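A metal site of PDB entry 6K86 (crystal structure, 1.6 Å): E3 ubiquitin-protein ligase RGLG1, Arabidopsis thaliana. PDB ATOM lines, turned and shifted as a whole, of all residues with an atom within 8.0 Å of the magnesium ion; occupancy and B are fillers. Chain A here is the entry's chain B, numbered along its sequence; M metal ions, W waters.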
ATOM      1  N   ASP A  44     -26.730  26.948 -12.902  1.00  0.00           N
ATOM      2  CA  ASP A  44     -27.379  25.809 -13.543  1.00  0.00           C
ATOM      3  C   ASP A  44     -26.397  24.655 -13.756  1.00  0.00           C
ATOM      4  O   ASP A  44     -25.407  24.805 -14.471  1.00  0.00           O
ATOM      5  CB  ASP A  44     -27.950  26.304 -14.874  1.00  0.00           C
ATOM      6  CG  ASP A  44     -28.586  25.222 -15.714  1.00  0.00           C
ATOM      7  OD1 ASP A  44     -28.154  24.052 -15.717  1.00  0.00           O
ATOM      8  OD2 ASP A  44     -29.519  25.558 -16.466  1.00  0.00           O
ATOM      9  N   PHE A  45     -26.678  23.498 -13.145  1.00  0.00           N
ATOM     10  CA  PHE A  45     -25.800  22.340 -13.261  1.00  0.00           C
ATOM     11  C   PHE A  45     -26.541  21.157 -13.884  1.00  0.00           C
ATOM     12  O   PHE A  45     -26.375  20.009 -13.438  1.00  0.00           O
ATOM     13  CB  PHE A  45     -25.215  21.962 -11.907  1.00  0.00           C
ATOM     14  CG  PHE A  45     -24.172  22.910 -11.387  1.00  0.00           C
ATOM     15  CD1 PHE A  45     -22.987  23.101 -12.060  1.00  0.00           C
ATOM     16  CD2 PHE A  45     -24.372  23.592 -10.187  1.00  0.00           C
ATOM     17  CE1 PHE A  45     -22.004  23.966 -11.572  1.00  0.00           C
ATOM     18  CE2 PHE A  45     -23.406  24.455  -9.671  1.00  0.00           C
ATOM     19  CZ  PHE A  45     -22.220  24.646 -10.361  1.00  0.00           C
ATOM     20  N   THR A  46     -27.384  21.446 -14.870  1.00  0.00           N
ATOM     21  CA  THR A  46     -28.167  20.411 -15.559  1.00  0.00           C
ATOM     22  C   THR A  46     -27.296  19.720 -16.605  1.00  0.00           C
ATOM     23  O   THR A  46     -26.302  20.292 -17.075  1.00  0.00           O
ATOM     24  CB  THR A  46     -29.422  20.985 -16.237  1.00  0.00           C
ATOM     25  OG1 THR A  46     -29.058  21.979 -17.203  1.00  0.00           O
ATOM     26  CG2 THR A  46     -30.366  21.578 -15.193  1.00  0.00           C
ATOM     27  N   LYS A  47     -27.689  18.509 -16.960  1.00  0.00           N
ATOM     28  CA  LYS A  47     -26.880  17.651 -17.826  1.00  0.00           C
ATOM     29  C   LYS A  47     -26.812  18.192 -19.250  1.00  0.00           C
ATOM     30  O   LYS A  47     -25.883  17.892 -19.997  1.00  0.00           O
ATOM     31  CB  LYS A  47     -27.420  16.227 -17.815  1.00  0.00           C
ATOM     32  CG  LYS A  47     -26.438  15.200 -18.358  1.00  0.00           C
ATOM     33  CD  LYS A  47     -26.749  13.786 -17.891  1.00  0.00           C
ATOM     34  CE  LYS A  47     -25.645  12.836 -18.313  1.00  0.00           C
ATOM     35  NZ  LYS A  47     -25.452  12.936 -19.783  1.00  0.00           N
ATOM     36  N   SER A  48     -27.795  18.999 -19.616  1.00  0.00           N
ATOM     37  CA  SER A  48     -27.829  19.599 -20.947  1.00  0.00           C
ATOM     38  C   SER A  48     -26.589  20.445 -21.222  1.00  0.00           C
ATOM     39  O   SER A  48     -26.190  20.602 -22.383  1.00  0.00           O
ATOM     40  CB  SER A  48     -29.089  20.458 -21.102  1.00  0.00           C
ATOM     41  OG  SER A  48     -29.027  21.582 -20.253  1.00  0.00           O
ATOM     42  N   ASN A  49     -25.955  20.957 -20.176  1.00  0.00           N
ATOM     43  CA  ASN A  49     -24.707  21.696 -20.318  1.00  0.00           C
ATOM     44  C   ASN A  49     -23.657  20.926 -21.120  1.00  0.00           C
ATOM     45  O   ASN A  49     -22.761  21.526 -21.709  1.00  0.00           O
ATOM     46  CB  ASN A  49     -24.143  22.056 -18.942  1.00  0.00           C
ATOM     47  CG  ASN A  49     -24.826  23.266 -18.321  1.00  0.00           C
ATOM     48  OD1 ASN A  49     -24.589  24.403 -18.753  1.00  0.00           O
ATOM     49  ND2 ASN A  49     -25.656  23.030 -17.304  1.00  0.00           N
ATOM     50  N   GLU A  50     -23.800  19.608 -21.152  1.00  0.00           N
ATOM     51  CA  GLU A  50     -22.849  18.781 -21.878  1.00  0.00           C
ATOM     52  C   GLU A  50     -22.936  18.997 -23.394  1.00  0.00           C
ATOM     53  O   GLU A  50     -21.912  18.938 -24.081  1.00  0.00           O
ATOM     54  CB  GLU A  50     -23.074  17.305 -21.528  1.00  0.00           C
ATOM     55  CG  GLU A  50     -22.577  17.001 -20.127  1.00  0.00           C
ATOM     56  CD  GLU A  50     -22.674  15.526 -19.751  1.00  0.00           C
ATOM     57  OE1 GLU A  50     -22.263  15.208 -18.617  1.00  0.00           O
ATOM     58  OE2 GLU A  50     -23.165  14.713 -20.561  1.00  0.00           O
ATOM     59  N   TRP A  51     -24.121  19.289 -23.919  1.00  0.00           N
ATOM     60  CA  TRP A  51     -24.270  19.426 -25.362  1.00  0.00           C
ATOM     61  C   TRP A  51     -24.726  20.801 -25.883  1.00  0.00           C
ATOM     62  O   TRP A  51     -24.782  21.008 -27.109  1.00  0.00           O
ATOM     63  CB  TRP A  51     -25.231  18.355 -25.891  1.00  0.00           C
ATOM     64  CG  TRP A  51     -26.591  18.396 -25.286  1.00  0.00           C
ATOM     65  CD1 TRP A  51     -27.635  19.200 -25.670  1.00  0.00           C
ATOM     66  CD2 TRP A  51     -27.089  17.579 -24.216  1.00  0.00           C
ATOM     67  NE1 TRP A  51     -28.745  18.941 -24.883  1.00  0.00           N
ATOM     68  CE2 TRP A  51     -28.433  17.948 -23.984  1.00  0.00           C
ATOM     69  CE3 TRP A  51     -26.526  16.580 -23.416  1.00  0.00           C
ATOM     70  CZ2 TRP A  51     -29.217  17.344 -23.006  1.00  0.00           C
ATOM     71  CZ3 TRP A  51     -27.308  15.984 -22.432  1.00  0.00           C
ATOM     72  CH2 TRP A  51     -28.642  16.374 -22.236  1.00  0.00           C
ATOM     73  N   THR A  52     -25.031  21.737 -24.998  1.00  0.00           N
ATOM     74  CA  THR A  52     -25.454  23.063 -25.465  1.00  0.00           C
ATOM     75  C   THR A  52     -24.257  23.950 -25.777  1.00  0.00           C
ATOM     76  O   THR A  52     -24.402  25.132 -26.063  1.00  0.00           O
ATOM     77  CB  THR A  52     -26.339  23.794 -24.449  1.00  0.00           C
ATOM     78  OG1 THR A  52     -25.681  23.826 -23.176  1.00  0.00           O
ATOM     79  CG2 THR A  52     -27.682  23.081 -24.315  1.00  0.00           C
ATOM     80  N   LEU A  62     -20.343  23.195 -21.242  1.00  0.00           N
ATOM     81  CA  LEU A  62     -20.341  24.582 -20.800  1.00  0.00           C
ATOM     82  C   LEU A  62     -19.654  24.724 -19.446  1.00  0.00           C
ATOM     83  O   LEU A  62     -19.224  25.814 -19.062  1.00  0.00           O
ATOM     84  CB  LEU A  62     -21.769  25.116 -20.729  1.00  0.00           C
ATOM     85  CG  LEU A  62     -22.492  25.285 -22.059  1.00  0.00           C
ATOM     86  CD1 LEU A  62     -23.834  25.942 -21.824  1.00  0.00           C
ATOM     87  CD2 LEU A  62     -21.680  26.124 -23.025  1.00  0.00           C
ATOM     88  N   TYR A  72     -19.813  30.248 -17.907  1.00  0.00           N
ATOM     89  CA  TYR A  72     -20.228  30.550 -16.543  1.00  0.00           C
ATOM     90  C   TYR A  72     -19.215  31.438 -15.847  1.00  0.00           C
ATOM     91  O   TYR A  72     -19.570  32.451 -15.233  1.00  0.00           O
ATOM     92  CB  TYR A  72     -20.454  29.263 -15.733  1.00  0.00           C
ATOM     93  CG  TYR A  72     -21.713  28.535 -16.152  1.00  0.00           C
ATOM     94  CD1 TYR A  72     -22.938  28.835 -15.568  1.00  0.00           C
ATOM     95  CD2 TYR A  72     -21.690  27.583 -17.146  1.00  0.00           C
ATOM     96  CE1 TYR A  72     -24.090  28.178 -15.942  1.00  0.00           C
ATOM     97  CE2 TYR A  72     -22.844  26.918 -17.543  1.00  0.00           C
ATOM     98  CZ  TYR A  72     -24.056  27.234 -16.954  1.00  0.00           C
ATOM     99  OH  TYR A  72     -25.199  26.577 -17.368  1.00  0.00           O
ATOM    100  N   PHE A  97     -28.044  24.446  -8.756  1.00  0.00           N
ATOM    101  CA  PHE A  97     -29.291  23.720  -8.909  1.00  0.00           C
ATOM    102  C   PHE A  97     -29.236  22.923 -10.199  1.00  0.00           C
ATOM    103  O   PHE A  97     -28.496  23.272 -11.114  1.00  0.00           O
ATOM    104  CB  PHE A  97     -30.503  24.657  -8.945  1.00  0.00           C
ATOM    105  CG  PHE A  97     -30.454  25.663 -10.062  1.00  0.00           C
ATOM    106  CD1 PHE A  97     -29.833  26.881  -9.888  1.00  0.00           C
ATOM    107  CD2 PHE A  97     -31.049  25.377 -11.292  1.00  0.00           C
ATOM    108  CE1 PHE A  97     -29.783  27.798 -10.914  1.00  0.00           C
ATOM    109  CE2 PHE A  97     -30.988  26.302 -12.336  1.00  0.00           C
ATOM    110  CZ  PHE A  97     -30.348  27.511 -12.138  1.00  0.00           C
ATOM    111  N   GLY A  98     -30.033  21.853 -10.262  1.00  0.00           N
ATOM    112  CA  GLY A  98     -30.156  21.074 -11.470  1.00  0.00           C
ATOM    113  C   GLY A  98     -29.212  19.894 -11.514  1.00  0.00           C
ATOM    114  O   GLY A  98     -29.212  19.126 -12.489  1.00  0.00           O
ATOM    115  N   ALA A 137     -27.815  16.866 -13.778  1.00  0.00           N
ATOM    116  CA  ALA A 137     -29.124  16.216 -13.919  1.00  0.00           C
ATOM    117  C   ALA A 137     -30.168  17.158 -14.541  1.00  0.00           C
ATOM    118  O   ALA A 137     -29.933  17.760 -15.589  1.00  0.00           O
ATOM    119  CB  ALA A 137     -29.602  15.703 -12.586  1.00  0.00           C
ATOM    120  N   GLY A 138     -31.327  17.256 -13.900  1.00  0.00           N
ATOM    121  CA  GLY A 138     -32.392  18.139 -14.352  1.00  0.00           C
ATOM    122  C   GLY A 138     -33.635  17.787 -13.546  1.00  0.00           C
ATOM    123  O   GLY A 138     -33.524  17.142 -12.500  1.00  0.00           O
ATOM    124  N   PRO A 139     -34.818  18.211 -14.007  1.00  0.00           N
ATOM    125  CA  PRO A 139     -35.082  19.084 -15.159  1.00  0.00           C
ATOM    126  C   PRO A 139     -34.802  20.522 -14.766  1.00  0.00           C
ATOM    127  O   PRO A 139     -34.089  20.735 -13.785  1.00  0.00           O
ATOM    128  CB  PRO A 139     -36.566  18.843 -15.439  1.00  0.00           C
ATOM    129  CG  PRO A 139     -37.141  18.639 -14.065  1.00  0.00           C
ATOM    130  CD  PRO A 139     -36.064  17.838 -13.316  1.00  0.00           C
ATOM    131  N   THR A 140     -35.354  21.498 -15.484  1.00  0.00           N
ATOM    132  CA  THR A 140     -35.027  22.908 -15.239  1.00  0.00           C
ATOM    133  C   THR A 140     -36.192  23.713 -14.649  1.00  0.00           C
ATOM    134  O   THR A 140     -37.260  23.861 -15.280  1.00  0.00           O
ATOM    135  CB  THR A 140     -34.569  23.591 -16.552  1.00  0.00           C
ATOM    136  OG1 THR A 140     -33.446  22.903 -17.091  1.00  0.00           O
ATOM    137  CG2 THR A 140     -34.197  25.057 -16.320  1.00  0.00           C
ATOM    138  N   PHE A 142     -36.561  27.478 -12.157  1.00  0.00           N
ATOM    139  CA  PHE A 142     -35.894  28.532 -11.419  1.00  0.00           C
ATOM    140  C   PHE A 142     -36.650  28.867 -10.133  1.00  0.00           C
ATOM    141  O   PHE A 142     -36.306  29.801  -9.425  1.00  0.00           O
ATOM    142  CB  PHE A 142     -35.735  29.776 -12.297  1.00  0.00           C
ATOM    143  CG  PHE A 142     -35.002  29.502 -13.569  1.00  0.00           C
ATOM    144  CD1 PHE A 142     -33.836  28.743 -13.548  1.00  0.00           C
ATOM    145  CD2 PHE A 142     -35.502  29.937 -14.792  1.00  0.00           C
ATOM    146  CE1 PHE A 142     -33.159  28.473 -14.706  1.00  0.00           C
ATOM    147  CE2 PHE A 142     -34.820  29.660 -15.961  1.00  0.00           C
ATOM    148  CZ  PHE A 142     -33.654  28.923 -15.918  1.00  0.00           C
ATOM    149  N   ALA A 167     -27.912  30.144 -16.672  1.00  0.00           N
ATOM    150  CA  ALA A 167     -28.558  28.884 -17.029  1.00  0.00           C
ATOM    151  C   ALA A 167     -28.388  28.576 -18.520  1.00  0.00           C
ATOM    152  O   ALA A 167     -28.135  29.475 -19.310  1.00  0.00           O
ATOM    153  CB  ALA A 167     -30.054  28.941 -16.636  1.00  0.00           C
ATOM    154  N   ASP A 168     -28.509  27.302 -18.900  1.00  0.00           N
ATOM    155  CA  ASP A 168     -28.294  26.942 -20.300  1.00  0.00           C
ATOM    156  C   ASP A 168     -29.571  26.485 -20.976  1.00  0.00           C
ATOM    157  O   ASP A 168     -29.560  25.935 -22.070  1.00  0.00           O
ATOM    158  CB  ASP A 168     -27.204  25.860 -20.433  1.00  0.00           C
ATOM    159  CG  ASP A 168     -27.761  24.472 -20.228  1.00  0.00           C
ATOM    160  OD1 ASP A 168     -28.585  24.282 -19.299  1.00  0.00           O
ATOM    161  OD2 ASP A 168     -27.368  23.543 -20.984  1.00  0.00           O
ATOM    162  N   GLY A 169     -30.700  26.704 -20.322  1.00  0.00           N
ATOM    163  CA  GLY A 169     -31.968  26.416 -20.970  1.00  0.00           C
ATOM    164  C   GLY A 169     -33.124  27.111 -20.317  1.00  0.00           C
ATOM    165  O   GLY A 169     -33.049  27.535 -19.157  1.00  0.00           O
ATOM    166  N   GLN A 170     -34.214  27.227 -21.074  1.00  0.00           N
ATOM    167  CA  GLN A 170     -35.451  27.773 -20.548  1.00  0.00           C
ATOM    168  C   GLN A 170     -36.037  26.772 -19.552  1.00  0.00           C
ATOM    169  O   GLN A 170     -35.653  25.594 -19.557  1.00  0.00           O
ATOM    170  CB  GLN A 170     -36.431  28.080 -21.711  1.00  0.00           C
ATOM    171  CG  GLN A 170     -35.711  28.622 -22.988  1.00  0.00           C
ATOM    172  CD  GLN A 170     -36.636  28.994 -24.182  1.00  0.00           C
ATOM    173  OE1 GLN A 170     -37.230  30.071 -24.218  1.00  0.00           O
ATOM    174  NE2 GLN A 170     -36.702  28.106 -25.170  1.00  0.00           N
ATOM    175  N   THR A 172     -38.254  23.981 -18.070  1.00  0.00           N
ATOM    176  CA  THR A 172     -38.822  22.797 -18.724  1.00  0.00           C
ATOM    177  C   THR A 172     -40.304  22.999 -19.043  1.00  0.00           C
ATOM    178  O   THR A 172     -41.071  23.404 -18.182  1.00  0.00           O
ATOM    179  CB  THR A 172     -38.630  21.561 -17.851  1.00  0.00           C
ATOM    180  OG1 THR A 172     -37.221  21.345 -17.678  1.00  0.00           O
ATOM    181  CG2 THR A 172     -39.250  20.352 -18.534  1.00  0.00           C
ATOM    182  N   VAL A 208     -26.639  31.194 -21.275  1.00  0.00           N
ATOM    183  CA  VAL A 208     -25.365  30.802 -21.860  1.00  0.00           C
ATOM    184  C   VAL A 208     -25.596  29.584 -22.742  1.00  0.00           C
ATOM    185  O   VAL A 208     -26.638  28.927 -22.640  1.00  0.00           O
ATOM    186  CB  VAL A 208     -24.281  30.479 -20.798  1.00  0.00           C
ATOM    187  CG1 VAL A 208     -23.856  31.737 -20.052  1.00  0.00           C
ATOM    188  CG2 VAL A 208     -24.788  29.404 -19.809  1.00  0.00           C
ATOM    189  N   GLY A 211     -28.815  27.502 -26.369  1.00  0.00           N
ATOM    190  CA  GLY A 211     -30.247  27.631 -26.185  1.00  0.00           C
ATOM    191  C   GLY A 211     -30.993  26.360 -26.567  1.00  0.00           C
ATOM    192  O   GLY A 211     -30.534  25.253 -26.273  1.00  0.00           O
ATOM    193  N   TRP A 213     -33.128  30.005 -27.193  1.00  0.00           N
ATOM    194  CA  TRP A 213     -33.544  31.086 -26.317  1.00  0.00           C
ATOM    195  C   TRP A 213     -34.613  31.958 -26.972  1.00  0.00           C
ATOM    196  O   TRP A 213     -34.897  33.047 -26.504  1.00  0.00           O
ATOM    197  CB  TRP A 213     -32.355  31.965 -25.936  1.00  0.00           C
ATOM    198  CG  TRP A 213     -31.333  31.289 -25.101  1.00  0.00           C
ATOM    199  CD1 TRP A 213     -30.049  30.989 -25.459  1.00  0.00           C
ATOM    200  CD2 TRP A 213     -31.497  30.829 -23.747  1.00  0.00           C
ATOM    201  NE1 TRP A 213     -29.399  30.370 -24.409  1.00  0.00           N
ATOM    202  CE2 TRP A 213     -30.268  30.258 -23.353  1.00  0.00           C
ATOM    203  CE3 TRP A 213     -32.562  30.842 -22.845  1.00  0.00           C
ATOM    204  CZ2 TRP A 213     -30.076  29.710 -22.085  1.00  0.00           C
ATOM    205  CZ3 TRP A 213     -32.365  30.309 -21.584  1.00  0.00           C
ATOM    206  CH2 TRP A 213     -31.124  29.746 -21.207  1.00  0.00           C
HETATM  207 MG    MG M   1     -30.047  22.781 -19.043  1.00  0.00          MG
HETATM  208  O   HOH W   1     -31.265  24.107 -17.919  1.00  0.00           O
HETATM  209  O   HOH W   2     -31.705  20.993 -18.419  1.00  0.00           O
HETATM  210  O   HOH W   3     -31.350  23.025 -20.649  1.00  0.00           O
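The side-chain carboxylate of Asp 44 is in hydrogen-bond range of the backbone NH of Asp 168, at 3.2 Å. The side-chain carboxylate (OD1) of Asp 44 is in hydrogen-bond range of the backbone NH (N) of Thr 46 (2.8 Å). O of Ser 48 sits at hydrogen-bond distance from OG1 of Thr 52. OG1 of Thr 172 lies within hydrogen-bond range of N of Thr 140. OD2 of Asp 168 sits at hydrogen-bond distance from N of Asn 49 (3.1 Å). O of Asp 44 sits at hydrogen-bond distance from OH of Tyr 72. OD1 of Asp 44 is in hydrogen-bond range of ND2 of Asn 49 (3.1 Å). O of Thr 46 is in hydrogen-bond range of ND2 of Asn 49.
Asp 44 touches the magnesium ion (OD2 to MG, 3.8 Å). Thr 140 touches the magnesium ion. Five residues have an atom within 4 Å of the magnesium ion: Asp 44, Thr 46, Ser 48, Thr 140 and Asp 168.
The magnesium ion is bound by OG of Ser 48 (2.0 Å), water W3 (2.1 Å), OD1 of Asp 168 (2.1 Å), water W1 (2.1 Å), OG1 of Thr 46 (2.2 Å) and water W2 (2.5 Å).
Water W1 bridges the side-chain hydroxyl (OG1) of Thr 140 (2.6 Å) and the side-chain carboxylate (OD2) of Asp 44 (2.7 Å).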
